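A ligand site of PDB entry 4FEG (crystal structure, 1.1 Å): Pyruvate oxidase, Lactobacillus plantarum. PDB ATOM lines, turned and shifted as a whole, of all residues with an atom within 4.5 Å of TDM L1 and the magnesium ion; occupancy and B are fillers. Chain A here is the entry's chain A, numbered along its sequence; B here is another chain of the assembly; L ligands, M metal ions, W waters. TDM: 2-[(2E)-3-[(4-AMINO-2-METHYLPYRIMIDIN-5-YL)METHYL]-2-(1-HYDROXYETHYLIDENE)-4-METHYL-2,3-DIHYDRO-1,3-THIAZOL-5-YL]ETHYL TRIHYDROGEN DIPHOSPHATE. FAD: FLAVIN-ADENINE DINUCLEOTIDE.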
ATOM      1  N   ASN A  92       5.786 -21.836 -26.110  1.00  0.00           N
ATOM      2  CA  ASN A  92       5.502 -20.466 -25.724  1.00  0.00           C
ATOM      3  C   ASN A  92       4.036 -20.287 -25.306  1.00  0.00           C
ATOM      4  O   ASN A  92       3.740 -19.460 -24.476  1.00  0.00           O
ATOM      5  CB  ASN A  92       5.886 -19.479 -26.822  1.00  0.00           C
ATOM      6  CG  ASN A  92       7.360 -19.179 -26.745  1.00  0.00           C
ATOM      7  OD1 ASN A  92       8.171 -20.116 -26.668  1.00  0.00           O
ATOM      8  ND2 ASN A  92       7.754 -17.935 -26.737  1.00  0.00           N
ATOM      9  N   VAL A 394       2.781  -7.984 -27.784  1.00  0.00           N
ATOM     10  CA  VAL A 394       3.659  -7.596 -26.675  1.00  0.00           C
ATOM     11  C   VAL A 394       4.707  -6.610 -27.192  1.00  0.00           C
ATOM     12  O   VAL A 394       5.426  -6.885 -28.167  1.00  0.00           O
ATOM     13  CB  VAL A 394       4.338  -8.858 -26.083  1.00  0.00           C
ATOM     14  CG1 VAL A 394       5.472  -8.510 -25.145  1.00  0.00           C
ATOM     15  CG2 VAL A 394       3.309  -9.716 -25.410  1.00  0.00           C
ATOM     16  N   GLY A 395       4.804  -5.451 -26.524  1.00  0.00           N
ATOM     17  CA  GLY A 395       5.727  -4.424 -26.883  1.00  0.00           C
ATOM     18  C   GLY A 395       5.131  -3.060 -26.580  1.00  0.00           C
ATOM     19  O   GLY A 395       4.280  -2.919 -25.685  1.00  0.00           O
ATOM     20  N   ASP A 396       5.540  -2.034 -27.348  1.00  0.00           N
ATOM     21  CA  ASP A 396       4.946  -0.742 -27.162  1.00  0.00           C
ATOM     22  C   ASP A 396       3.428  -0.769 -27.301  1.00  0.00           C
ATOM     23  O   ASP A 396       2.772   0.080 -26.693  1.00  0.00           O
ATOM     24  CB  ASP A 396       5.514   0.252 -28.151  1.00  0.00           C
ATOM     25  CG  ASP A 396       6.841   0.863 -27.855  1.00  0.00           C
ATOM     26  OD1 ASP A 396       7.329   0.755 -26.745  1.00  0.00           O
ATOM     27  OD2 ASP A 396       7.383   1.532 -28.818  1.00  0.00           O
ATOM     28  N   ILE A 397       2.863  -1.716 -28.031  1.00  0.00           N
ATOM     29  CA  ILE A 397       1.408  -1.743 -28.165  1.00  0.00           C
ATOM     30  C   ILE A 397       0.739  -1.898 -26.815  1.00  0.00           C
ATOM     31  O   ILE A 397      -0.369  -1.364 -26.608  1.00  0.00           O
ATOM     32  CB  ILE A 397       0.939  -2.835 -29.168  1.00  0.00           C
ATOM     33  CG1 ILE A 397      -0.544  -2.702 -29.473  1.00  0.00           C
ATOM     34  CG2 ILE A 397       1.249  -4.239 -28.691  1.00  0.00           C
ATOM     35  CD1 ILE A 397      -0.997  -1.329 -30.025  1.00  0.00           C
ATOM     36  N   ALA A 420       4.604 -12.832 -21.158  1.00  0.00           N
ATOM     37  CA  ALA A 420       4.776 -11.796 -22.154  1.00  0.00           C
ATOM     38  C   ALA A 420       5.437 -12.311 -23.404  1.00  0.00           C
ATOM     39  O   ALA A 420       6.362 -11.710 -23.951  1.00  0.00           O
ATOM     40  CB  ALA A 420       5.483 -10.580 -21.601  1.00  0.00           C
ATOM     41  N   THR A 421       4.921 -13.438 -23.933  1.00  0.00           N
ATOM     42  CA  THR A 421       5.403 -13.916 -25.230  1.00  0.00           C
ATOM     43  C   THR A 421       4.855 -13.048 -26.377  1.00  0.00           C
ATOM     44  O   THR A 421       3.664 -12.909 -26.556  1.00  0.00           O
ATOM     45  CB  THR A 421       5.138 -15.402 -25.471  1.00  0.00           C
ATOM     46  OG1 THR A 421       5.706 -15.785 -26.710  1.00  0.00           O
ATOM     47  CG2 THR A 421       3.646 -15.778 -25.433  1.00  0.00           C
ATOM     48  N   MET A 422       5.798 -12.528 -27.171  1.00  0.00           N
ATOM     49  CA  MET A 422       5.421 -11.937 -28.440  1.00  0.00           C
ATOM     50  C   MET A 422       4.760 -13.022 -29.312  1.00  0.00           C
ATOM     51  O   MET A 422       5.002 -14.230 -29.142  1.00  0.00           O
ATOM     52  CB  MET A 422       6.658 -11.412 -29.146  1.00  0.00           C
ATOM     53  CG  MET A 422       7.298 -10.185 -28.495  1.00  0.00           C
ATOM     54  SD  MET A 422       8.934  -9.874 -29.120  1.00  0.00           S
ATOM     55  CE  MET A 422       8.628  -9.475 -30.839  1.00  0.00           C
ATOM     56  N   GLY A 446       2.671  -5.105 -32.735  1.00  0.00           N
ATOM     57  CA  GLY A 446       3.845  -4.535 -33.323  1.00  0.00           C
ATOM     58  C   GLY A 446       4.372  -5.384 -34.449  1.00  0.00           C
ATOM     59  O   GLY A 446       4.025  -6.573 -34.583  1.00  0.00           O
ATOM     60  N   ASP A 447       5.265  -4.814 -35.236  1.00  0.00           N
ATOM     61  CA  ASP A 447       5.841  -5.541 -36.362  1.00  0.00           C
ATOM     62  C   ASP A 447       6.700  -6.718 -35.938  1.00  0.00           C
ATOM     63  O   ASP A 447       6.692  -7.780 -36.572  1.00  0.00           O
ATOM     64  CB  ASP A 447       6.612  -4.617 -37.295  1.00  0.00           C
ATOM     65  CG  ASP A 447       7.634  -3.645 -36.752  1.00  0.00           C
ATOM     66  OD1 ASP A 447       7.825  -3.591 -35.495  1.00  0.00           O
ATOM     67  OD2 ASP A 447       8.208  -2.935 -37.591  1.00  0.00           O
ATOM     68  N   GLY A 448       7.431  -6.605 -34.823  1.00  0.00           N
ATOM     69  CA  GLY A 448       8.210  -7.710 -34.345  1.00  0.00           C
ATOM     70  C   GLY A 448       7.381  -8.913 -33.964  1.00  0.00           C
ATOM     71  O   GLY A 448       7.662 -10.068 -34.339  1.00  0.00           O
ATOM     72  N   GLY A 449       6.321  -8.658 -33.181  1.00  0.00           N
ATOM     73  CA  GLY A 449       5.440  -9.712 -32.705  1.00  0.00           C
ATOM     74  C   GLY A 449       4.582 -10.300 -33.833  1.00  0.00           C
ATOM     75  O   GLY A 449       4.445 -11.519 -33.923  1.00  0.00           O
ATOM     76  N   MET A 452       6.526 -12.796 -35.861  1.00  0.00           N
ATOM     77  CA  MET A 452       6.780 -14.105 -35.274  1.00  0.00           C
ATOM     78  C   MET A 452       5.685 -15.094 -35.590  1.00  0.00           C
ATOM     79  O   MET A 452       6.011 -16.287 -35.687  1.00  0.00           O
ATOM     80  CB  MET A 452       6.979 -13.985 -33.750  1.00  0.00           C
ATOM     81  CG  MET A 452       8.352 -13.388 -33.439  1.00  0.00           C
ATOM     82  SD  MET A 452       8.576 -13.294 -31.672  1.00  0.00           S
ATOM     83  CE  MET A 452      10.247 -12.626 -31.632  1.00  0.00           C
ATOM     84  N   PHE A 472       1.702  -2.359 -36.232  1.00  0.00           N
ATOM     85  CA  PHE A 472       2.368  -1.080 -35.942  1.00  0.00           C
ATOM     86  C   PHE A 472       3.826  -1.208 -36.387  1.00  0.00           C
ATOM     87  O   PHE A 472       4.660  -1.773 -35.691  1.00  0.00           O
ATOM     88  CB  PHE A 472       2.254  -0.731 -34.443  1.00  0.00           C
ATOM     89  CG  PHE A 472       0.843  -0.445 -33.999  1.00  0.00           C
ATOM     90  CD1 PHE A 472      -0.161  -1.375 -33.932  1.00  0.00           C
ATOM     91  CD2 PHE A 472       0.522   0.875 -33.681  1.00  0.00           C
ATOM     92  CE1 PHE A 472      -1.433  -1.064 -33.585  1.00  0.00           C
ATOM     93  CE2 PHE A 472      -0.732   1.214 -33.262  1.00  0.00           C
ATOM     94  CZ  PHE A 472      -1.747   0.264 -33.240  1.00  0.00           C
ATOM     95  N   ASN A 474       7.199   0.053 -36.974  1.00  0.00           N
ATOM     96  CA  ASN A 474       8.226   1.039 -36.677  1.00  0.00           C
ATOM     97  C   ASN A 474       9.600   0.572 -37.160  1.00  0.00           C
ATOM     98  O   ASN A 474      10.561   1.332 -36.982  1.00  0.00           O
ATOM     99  CB  ASN A 474       8.278   1.423 -35.215  1.00  0.00           C
ATOM    100  CG  ASN A 474       8.278   0.262 -34.284  1.00  0.00           C
ATOM    101  OD1 ASN A 474       8.563  -0.867 -34.645  1.00  0.00           O
ATOM    102  ND2 ASN A 474       8.028   0.549 -32.990  1.00  0.00           N
ATOM    103  N   GLN A 476      11.388  -1.528 -35.720  1.00  0.00           N
ATOM    104  CA  GLN A 476      12.133  -1.607 -34.497  1.00  0.00           C
ATOM    105  C   GLN A 476      11.519  -2.641 -33.567  1.00  0.00           C
ATOM    106  O   GLN A 476      10.297  -2.901 -33.631  1.00  0.00           O
ATOM    107  CB  GLN A 476      12.137  -0.280 -33.736  1.00  0.00           C
ATOM    108  CG  GLN A 476      12.697   0.870 -34.471  1.00  0.00           C
ATOM    109  CD  GLN A 476      12.476   2.184 -33.739  1.00  0.00           C
ATOM    110  OE1 GLN A 476      11.598   2.298 -32.913  1.00  0.00           O
ATOM    111  NE2 GLN A 476      13.287   3.148 -33.984  1.00  0.00           N
ATOM    112  N   TYR A 477      12.319  -3.102 -32.641  1.00  0.00           N
ATOM    113  CA  TYR A 477      11.818  -3.637 -31.354  1.00  0.00           C
ATOM    114  C   TYR A 477      11.778  -2.426 -30.423  1.00  0.00           C
ATOM    115  O   TYR A 477      12.716  -2.202 -29.648  1.00  0.00           O
ATOM    116  CB  TYR A 477      12.709  -4.728 -30.803  1.00  0.00           C
ATOM    117  CG  TYR A 477      12.791  -5.998 -31.662  1.00  0.00           C
ATOM    118  CD1 TYR A 477      11.651  -6.678 -32.041  1.00  0.00           C
ATOM    119  CD2 TYR A 477      14.011  -6.490 -32.068  1.00  0.00           C
ATOM    120  CE1 TYR A 477      11.732  -7.824 -32.812  1.00  0.00           C
ATOM    121  CE2 TYR A 477      14.067  -7.635 -32.855  1.00  0.00           C
ATOM    122  CZ  TYR A 477      12.939  -8.311 -33.224  1.00  0.00           C
ATOM    123  OH  TYR A 477      13.033  -9.418 -34.023  1.00  0.00           O
ATOM    124  N   GLY A 478      10.783  -1.583 -30.577  1.00  0.00           N
ATOM    125  CA  GLY A 478      10.795  -0.279 -29.942  1.00  0.00           C
ATOM    126  C   GLY A 478      10.887  -0.336 -28.448  1.00  0.00           C
ATOM    127  O   GLY A 478      11.671   0.403 -27.809  1.00  0.00           O
ATOM    128  N   PHE A 479      10.109  -1.254 -27.846  1.00  0.00           N
ATOM    129  CA  PHE A 479      10.129  -1.381 -26.398  1.00  0.00           C
ATOM    130  C   PHE A 479      11.535  -1.632 -25.890  1.00  0.00           C
ATOM    131  O   PHE A 479      11.909  -1.200 -24.805  1.00  0.00           O
ATOM    132  CB  PHE A 479       9.168  -2.520 -26.037  1.00  0.00           C
ATOM    133  CG  PHE A 479       8.588  -2.512 -24.649  1.00  0.00           C
ATOM    134  CD1 PHE A 479       7.593  -1.602 -24.293  1.00  0.00           C
ATOM    135  CD2 PHE A 479       8.994  -3.439 -23.690  1.00  0.00           C
ATOM    136  CE1 PHE A 479       7.009  -1.699 -23.004  1.00  0.00           C
ATOM    137  CE2 PHE A 479       8.428  -3.500 -22.446  1.00  0.00           C
ATOM    138  CZ  PHE A 479       7.430  -2.617 -22.105  1.00  0.00           C
ATOM    139  N   ILE A 480      12.313  -2.428 -26.658  1.00  0.00           N
ATOM    140  CA  ILE A 480      13.670  -2.801 -26.271  1.00  0.00           C
ATOM    141  C   ILE A 480      14.695  -1.728 -26.631  1.00  0.00           C
ATOM    142  O   ILE A 480      15.645  -1.488 -25.887  1.00  0.00           O
ATOM    143  CB  ILE A 480      14.079  -4.148 -26.884  1.00  0.00           C
ATOM    144  CG1 ILE A 480      13.033  -5.220 -26.602  1.00  0.00           C
ATOM    145  CG2 ILE A 480      15.461  -4.577 -26.406  1.00  0.00           C
ATOM    146  CD1 ILE A 480      12.666  -5.326 -25.164  1.00  0.00           C
ATOM    147  N   ILE B  32      17.682 -12.329 -30.455  1.00  0.00           N
ATOM    148  CA  ILE B  32      16.794 -11.164 -30.408  1.00  0.00           C
ATOM    149  C   ILE B  32      16.991 -10.525 -29.037  1.00  0.00           C
ATOM    150  O   ILE B  32      16.969 -11.261 -28.033  1.00  0.00           O
ATOM    151  CB  ILE B  32      15.314 -11.552 -30.634  1.00  0.00           C
ATOM    152  CG1 ILE B  32      15.135 -12.010 -32.080  1.00  0.00           C
ATOM    153  CG2 ILE B  32      14.335 -10.434 -30.239  1.00  0.00           C
ATOM    154  CD1 ILE B  32      13.746 -12.538 -32.405  1.00  0.00           C
ATOM    155  N   PRO B  33      17.216  -9.229 -28.961  1.00  0.00           N
ATOM    156  CA  PRO B  33      17.508  -8.598 -27.659  1.00  0.00           C
ATOM    157  C   PRO B  33      16.253  -8.498 -26.806  1.00  0.00           C
ATOM    158  O   PRO B  33      15.131  -8.585 -27.252  1.00  0.00           O
ATOM    159  CB  PRO B  33      18.045  -7.223 -28.033  1.00  0.00           C
ATOM    160  CG  PRO B  33      17.259  -6.911 -29.270  1.00  0.00           C
ATOM    161  CD  PRO B  33      17.215  -8.247 -30.025  1.00  0.00           C
ATOM    162  N   GLU B  59      13.388 -16.466 -32.495  1.00  0.00           N
ATOM    163  CA  GLU B  59      14.564 -17.108 -31.882  1.00  0.00           C
ATOM    164  C   GLU B  59      14.766 -18.546 -32.312  1.00  0.00           C
ATOM    165  O   GLU B  59      15.894 -19.041 -32.247  1.00  0.00           O
ATOM    166  CB  GLU B  59      14.501 -16.992 -30.371  1.00  0.00           C
ATOM    167  CG  GLU B  59      14.469 -15.582 -29.851  1.00  0.00           C
ATOM    168  CD  GLU B  59      13.101 -14.971 -29.680  1.00  0.00           C
ATOM    169  OE1 GLU B  59      12.095 -15.485 -30.237  1.00  0.00           O
ATOM    170  OE2 GLU B  59      13.033 -13.923 -28.984  1.00  0.00           O
ATOM    171  N   SER B  82      16.062 -14.027 -24.931  1.00  0.00           N
ATOM    172  CA  SER B  82      15.696 -13.276 -23.753  1.00  0.00           C
ATOM    173  C   SER B  82      14.935 -14.136 -22.772  1.00  0.00           C
ATOM    174  O   SER B  82      14.403 -15.211 -23.084  1.00  0.00           O
ATOM    175  CB  SER B  82      14.874 -12.040 -24.187  1.00  0.00           C
ATOM    176  OG  SER B  82      13.682 -12.406 -24.879  1.00  0.00           O
ATOM    177  N   PRO B  85      10.055 -16.174 -22.820  1.00  0.00           N
ATOM    178  CA  PRO B  85       9.700 -16.576 -24.182  1.00  0.00           C
ATOM    179  C   PRO B  85      10.792 -16.483 -25.196  1.00  0.00           C
ATOM    180  O   PRO B  85      10.684 -17.166 -26.245  1.00  0.00           O
ATOM    181  CB  PRO B  85       8.554 -15.599 -24.537  1.00  0.00           C
ATOM    182  CG  PRO B  85       8.800 -14.396 -23.656  1.00  0.00           C
ATOM    183  CD  PRO B  85       9.207 -15.042 -22.358  1.00  0.00           C
ATOM    184  N   GLY B  86      11.800 -15.663 -25.030  1.00  0.00           N
ATOM    185  CA  GLY B  86      12.899 -15.672 -25.987  1.00  0.00           C
ATOM    186  C   GLY B  86      13.620 -17.022 -25.979  1.00  0.00           C
ATOM    187  O   GLY B  86      13.825 -17.650 -27.012  1.00  0.00           O
ATOM    188  N   HIS B  89      11.550 -20.117 -27.159  1.00  0.00           N
ATOM    189  CA  HIS B  89      11.512 -20.178 -28.620  1.00  0.00           C
ATOM    190  C   HIS B  89      12.722 -20.897 -29.235  1.00  0.00           C
ATOM    191  O   HIS B  89      12.660 -21.303 -30.393  1.00  0.00           O
ATOM    192  CB  HIS B  89      11.416 -18.786 -29.226  1.00  0.00           C
ATOM    193  CG  HIS B  89      10.042 -18.327 -29.556  1.00  0.00           C
ATOM    194  ND1 HIS B  89       9.819 -17.053 -30.029  1.00  0.00           N
ATOM    195  CD2 HIS B  89       8.838 -18.936 -29.621  1.00  0.00           C
ATOM    196  CE1 HIS B  89       8.531 -16.918 -30.340  1.00  0.00           C
ATOM    197  NE2 HIS B  89       7.900 -18.065 -30.100  1.00  0.00           N
ATOM    198  N   PHE B 121       8.186  -9.459 -13.283  1.00  0.00           N
ATOM    199  CA  PHE B 121       7.730  -9.593 -14.645  1.00  0.00           C
ATOM    200  C   PHE B 121       8.620 -10.508 -15.433  1.00  0.00           C
ATOM    201  O   PHE B 121       9.836 -10.347 -15.439  1.00  0.00           O
ATOM    202  CB  PHE B 121       7.741  -8.198 -15.280  1.00  0.00           C
ATOM    203  CG  PHE B 121       7.366  -8.196 -16.715  1.00  0.00           C
ATOM    204  CD1 PHE B 121       6.084  -8.308 -17.142  1.00  0.00           C
ATOM    205  CD2 PHE B 121       8.336  -8.058 -17.678  1.00  0.00           C
ATOM    206  CE1 PHE B 121       5.733  -8.304 -18.486  1.00  0.00           C
ATOM    207  CE2 PHE B 121       8.026  -8.057 -19.024  1.00  0.00           C
ATOM    208  CZ  PHE B 121       6.699  -8.167 -19.425  1.00  0.00           C
ATOM    209  N   GLN B 122       7.961 -11.515 -16.017  1.00  0.00           N
ATOM    210  CA  GLN B 122       8.666 -12.459 -16.914  1.00  0.00           C
ATOM    211  C   GLN B 122       9.855 -13.107 -16.213  1.00  0.00           C
ATOM    212  O   GLN B 122      10.854 -13.483 -16.812  1.00  0.00           O
ATOM    213  CB  GLN B 122       9.027 -11.733 -18.201  1.00  0.00           C
ATOM    214  CG  GLN B 122       9.416 -12.677 -19.310  1.00  0.00           C
ATOM    215  CD  GLN B 122       9.891 -11.796 -20.426  1.00  0.00           C
ATOM    216  OE1 GLN B 122      10.989 -11.267 -20.259  1.00  0.00           O
ATOM    217  NE2 GLN B 122       9.124 -11.622 -21.488  1.00  0.00           N
HETATM  218  O1A TDM L   1       8.068  -4.604 -32.915  1.00  0.00           O
HETATM  219  PA  TDM L   1       7.522  -5.100 -31.604  1.00  0.00           P
HETATM  220  O2A TDM L   1       6.557  -6.231 -31.682  1.00  0.00           O
HETATM  221  O3A TDM L   1       6.823  -3.911 -30.812  1.00  0.00           O
HETATM  222  PB  TDM L   1       7.252  -2.333 -30.645  1.00  0.00           P
HETATM  223  O2B TDM L   1       8.300  -2.053 -31.689  1.00  0.00           O
HETATM  224  O3B TDM L   1       7.738  -2.179 -29.243  1.00  0.00           O
HETATM  225  O1B TDM L   1       5.943  -1.648 -30.940  1.00  0.00           O
HETATM  226  O7  TDM L   1       8.777  -5.452 -30.705  1.00  0.00           O
HETATM  227  C7  TDM L   1       8.587  -6.054 -29.391  1.00  0.00           C
HETATM  228  C6  TDM L   1       9.945  -5.963 -28.721  1.00  0.00           C
HETATM  229  C5  TDM L   1      10.037  -6.816 -27.459  1.00  0.00           C
HETATM  230  S1  TDM L   1       9.008  -6.450 -26.087  1.00  0.00           S
HETATM  231  C2  TDM L   1       9.567  -7.831 -25.220  1.00  0.00           C
HETATM  232  C27 TDM L   1       9.537  -7.747 -23.702  1.00  0.00           C
HETATM  233  C29 TDM L   1       8.272  -7.029 -23.217  1.00  0.00           C
HETATM  234  O28 TDM L   1       9.575  -9.034 -23.147  1.00  0.00           O
HETATM  235  N3  TDM L   1      10.697  -8.374 -25.922  1.00  0.00           N
HETATM  236  C4  TDM L   1      10.858  -7.824 -27.199  1.00  0.00           C
HETATM  237  CM4 TDM L   1      11.943  -8.379 -28.111  1.00  0.00           C
HETATM  238  C7' TDM L   1      11.398  -9.634 -25.479  1.00  0.00           C
HETATM  239  C5' TDM L   1      10.857 -10.887 -26.187  1.00  0.00           C
HETATM  240  C4' TDM L   1       9.519 -11.392 -25.897  1.00  0.00           C
HETATM  241  N4' TDM L   1       8.735 -10.853 -24.984  1.00  0.00           N
HETATM  242  N3' TDM L   1       9.043 -12.494 -26.579  1.00  0.00           N
HETATM  243  C2' TDM L   1       9.895 -13.109 -27.438  1.00  0.00           C
HETATM  244  CM2 TDM L   1       9.407 -14.328 -28.176  1.00  0.00           C
HETATM  245  N1' TDM L   1      11.138 -12.728 -27.631  1.00  0.00           N
HETATM  246  C6' TDM L   1      11.630 -11.586 -27.002  1.00  0.00           C
HETATM  247  PA  FAD L   2      -2.958 -11.604 -11.867  1.00  0.00           P
HETATM  248  O1A FAD L   2      -3.589 -12.669 -12.700  1.00  0.00           O
HETATM  249  O2A FAD L   2      -1.482 -11.603 -11.732  1.00  0.00           O
HETATM  250  O5B FAD L   2      -3.521 -11.620 -10.379  1.00  0.00           O
HETATM  251  C5B FAD L   2      -4.952 -11.733 -10.125  1.00  0.00           C
HETATM  252  C4B FAD L   2      -5.054 -11.761  -8.618  1.00  0.00           C
HETATM  253  O4B FAD L   2      -6.482 -11.824  -8.311  1.00  0.00           O
HETATM  254  C3B FAD L   2      -4.394 -13.034  -7.943  1.00  0.00           C
HETATM  255  O3B FAD L   2      -3.666 -12.637  -6.775  1.00  0.00           O
HETATM  256  C2B FAD L   2      -5.628 -13.870  -7.644  1.00  0.00           C
HETATM  257  O2B FAD L   2      -5.452 -14.806  -6.578  1.00  0.00           O
HETATM  258  C1B FAD L   2      -6.687 -12.851  -7.324  1.00  0.00           C
HETATM  259  N9A FAD L   2      -8.075 -13.324  -7.483  1.00  0.00           N
HETATM  260  C8A FAD L   2      -8.573 -14.056  -8.523  1.00  0.00           C
HETATM  261  N7A FAD L   2      -9.927 -14.203  -8.409  1.00  0.00           N
HETATM  262  C5A FAD L   2     -10.282 -13.498  -7.274  1.00  0.00           C
HETATM  263  C6A FAD L   2     -11.518 -13.260  -6.645  1.00  0.00           C
HETATM  264  N6A FAD L   2     -12.658 -13.777  -7.046  1.00  0.00           N
HETATM  265  N1A FAD L   2     -11.481 -12.446  -5.544  1.00  0.00           N
HETATM  266  C2A FAD L   2     -10.325 -11.963  -5.047  1.00  0.00           C
HETATM  267  N3A FAD L   2      -9.097 -12.160  -5.625  1.00  0.00           N
HETATM  268  C4A FAD L   2      -9.159 -12.928  -6.740  1.00  0.00           C
HETATM  269  N1  FAD L   2       1.096  -4.408 -15.669  1.00  0.00           N
HETATM  270  C2  FAD L   2       1.101  -3.198 -15.029  1.00  0.00           C
HETATM  271  O2  FAD L   2       0.151  -2.892 -14.258  1.00  0.00           O
HETATM  272  N3  FAD L   2       2.123  -2.322 -15.267  1.00  0.00           N
HETATM  273  C4  FAD L   2       3.133  -2.534 -16.154  1.00  0.00           C
HETATM  274  O4  FAD L   2       4.073  -1.683 -16.312  1.00  0.00           O
HETATM  275  C4X FAD L   2       3.097  -3.766 -16.871  1.00  0.00           C
HETATM  276  N5  FAD L   2       4.148  -4.134 -17.697  1.00  0.00           N
HETATM  277  C5X FAD L   2       3.807  -5.019 -18.706  1.00  0.00           C
HETATM  278  C6  FAD L   2       4.526  -5.082 -19.890  1.00  0.00           C
HETATM  279  C7  FAD L   2       4.198  -5.965 -20.926  1.00  0.00           C
HETATM  280  C7M FAD L   2       5.000  -5.974 -22.221  1.00  0.00           C
HETATM  281  C8  FAD L   2       3.081  -6.824 -20.735  1.00  0.00           C
HETATM  282  C8M FAD L   2       2.678  -7.793 -21.827  1.00  0.00           C
HETATM  283  C9  FAD L   2       2.385  -6.749 -19.539  1.00  0.00           C
HETATM  284  C9A FAD L   2       2.722  -5.897 -18.511  1.00  0.00           C
HETATM  285  N10 FAD L   2       2.019  -5.825 -17.267  1.00  0.00           N
HETATM  286  C10 FAD L   2       2.075  -4.660 -16.560  1.00  0.00           C
HETATM  287  C1' FAD L   2       1.207  -6.933 -16.772  1.00  0.00           C
HETATM  288  C2' FAD L   2       1.903  -7.549 -15.550  1.00  0.00           C
HETATM  289  O2' FAD L   2       3.045  -8.352 -16.003  1.00  0.00           O
HETATM  290  C3' FAD L   2       0.984  -8.395 -14.659  1.00  0.00           C
HETATM  291  O3' FAD L   2       0.387  -9.439 -15.476  1.00  0.00           O
HETATM  292  C4' FAD L   2      -0.176  -7.572 -14.116  1.00  0.00           C
HETATM  293  O4' FAD L   2       0.257  -6.302 -13.536  1.00  0.00           O
HETATM  294  C5' FAD L   2      -0.860  -8.370 -12.998  1.00  0.00           C
HETATM  295  O5' FAD L   2      -2.278  -8.082 -13.082  1.00  0.00           O
HETATM  296  P   FAD L   2      -3.313  -8.687 -12.059  1.00  0.00           P
HETATM  297  O1P FAD L   2      -2.830  -8.603 -10.675  1.00  0.00           O
HETATM  298  O2P FAD L   2      -4.609  -8.033 -12.425  1.00  0.00           O
HETATM  299  O3P FAD L   2      -3.452 -10.230 -12.492  1.00  0.00           O
HETATM  300 MG    MG M   1       8.255  -2.761 -33.700  1.00  0.00          MG
HETATM  301  O   HOH W   1       3.974  -3.345 -30.029  1.00  0.00           O
HETATM  302  O   HOH W   2       4.403   0.531 -31.643  1.00  0.00           O
HETATM  303  O   HOH W   3       4.116  -6.221 -30.547  1.00  0.00           O
HETATM  304  O   HOH W   4      11.777 -11.900 -23.052  1.00  0.00           O
HETATM  305  O   HOH W   5       6.208  -2.244 -33.598  1.00  0.00           O
HETATM  306  O   HOH W   6      11.163  -5.642 -21.650  1.00  0.00           O
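Val 394 touches TDM L1. Gly 395 touches TDM L1. CA of Gly 446 touches O2A of TDM L1 (3.6 Å). SD of Met 452 touches CM2 of TDM L1, at 3.7 Å. Tyr 477 touches TDM L1. CG1 of Ile 480 touches C4 of TDM L1, 3.4 Å away. Ile 32 of chain B touches TDM L1 (CG2 to CM4, 3.8 Å). Pro 33 of chain B touches TDM L1. Ser 82 of chain B touches TDM L1 (OG to C6', 3.1 Å). CG of Pro 85 of chain B touches N3' of TDM L1, 3.5 Å away. CA of Gly 86 of chain B touches N1' of TDM L1, at 3.8 Å. His 89 of chain B touches TDM L1. Hydrophobic or aromatic side chains that line TDM L1: Val 394, Met 422, Met 452, Tyr 477, Phe 479, Ile 480, Ile 32 of chain B, Pro 85 of chain B and His 89 of chain B. Within 4 Å of TDM L1: Val 394, Gly 395, Asp 396, Ala 420, Met 422, Gly 446, Asp 447, Gly 448, Gly 449, Met 452, Asn 474, Gln 476, Tyr 477, Gly 478, Phe 479, Ile 480, Ile 32 of chain B, Pro 33 of chain B, Glu 59 of chain B, Ser 82 of chain B, Pro 85 of chain B, Gly 86 of chain B, His 89 of chain B and Gln 122 of chain B. The nearest printed residue that does not touch TDM L1 is Thr 421 (4.1 Å).
The magnesium ion is bound by an oxygen (O1A) of TDM L1 (2.0 Å). The magnesium ion is bound by OD1 of Asp 447, at 2.0 Å. O of Gln 476 is bound to the magnesium ion (2.0 Å). Water W5 binds the magnesium ion (2.1 Å). An oxygen (O2B) of TDM L1 binds the magnesium ion (2.1 Å). OD1 of Asn 474 binds the magnesium ion (2.1 Å).
Water W5 lies within hydrogen-bond range of the backbone carbonyl oxygen (O) of Phe 472 (2.6 Å), an oxygen (O1B) of TDM L1 (2.7 Å), the backbone NH (N) of Asp 447 (3.2 Å) and the side-chain amide nitrogen (ND2) of Asn 474 (3.4 Å). Water W3 lies within hydrogen-bond range of O2A of TDM L1, O of Val 394 and N of Gly 446. Water W4 lies within hydrogen-bond range of the side-chain hydroxyl (OG) of Ser 82 of chain B and the side-chain amide oxygen (OE1) of Gln 122 of chain B.
The backbone carbonyl oxygen (O) of Pro 85 of chain B sits at hydrogen-bond distance from the side-chain amide nitrogen (ND2) of Asn 92, at 3.1 Å. A ring nitrogen (NE2) of His 89 of chain B lies close to the side-chain amide nitrogen of Asn 92 (3.4 Å). OE1 of Glu 59 of chain B is in hydrogen-bond range of ND1 of His 89 of chain B (2.8 Å). The backbone NH of Asp 447 sits at hydrogen-bond distance from the backbone carbonyl oxygen of Phe 472, 3.1 Å away.
The backbone NH of Asp 396 lies within hydrogen-bond range of an oxygen (O3B) of TDM L1, 2.9 Å away. The backbone NH (N) of Gly 448 sits at hydrogen-bond distance from an oxygen (O2A) of TDM L1 (3.3 Å). N1' of TDM L1 lies within hydrogen-bond range of OE2 of Glu 59 of chain B, 2.6 Å away. The backbone NH of Met 422 is in hydrogen-bond range of a nitrogen (N3') of TDM L1, 3.3 Å away. The backbone carbonyl oxygen (O) of Ala 420 lies within hydrogen-bond range of a nitrogen (N4') of TDM L1 (2.7 Å). N of Gly 478 sits at hydrogen-bond distance from O3B of TDM L1 (3.4 Å). NE2 of Gln 122 of chain B sits at hydrogen-bond distance from O28 of TDM L1 (3.1 Å). N of Phe 479 sits at hydrogen-bond distance from O3B of TDM L1 (2.9 Å). N of Gly 449 sits at hydrogen-bond distance from O2A of TDM L1 (2.9 Å).
Within 4 Å of the magnesium ion: Asp 447, Asn 474 and Gln 476. The nearest printed residue that does not touch the magnesium ion is Gly 448 (4.1 Å).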
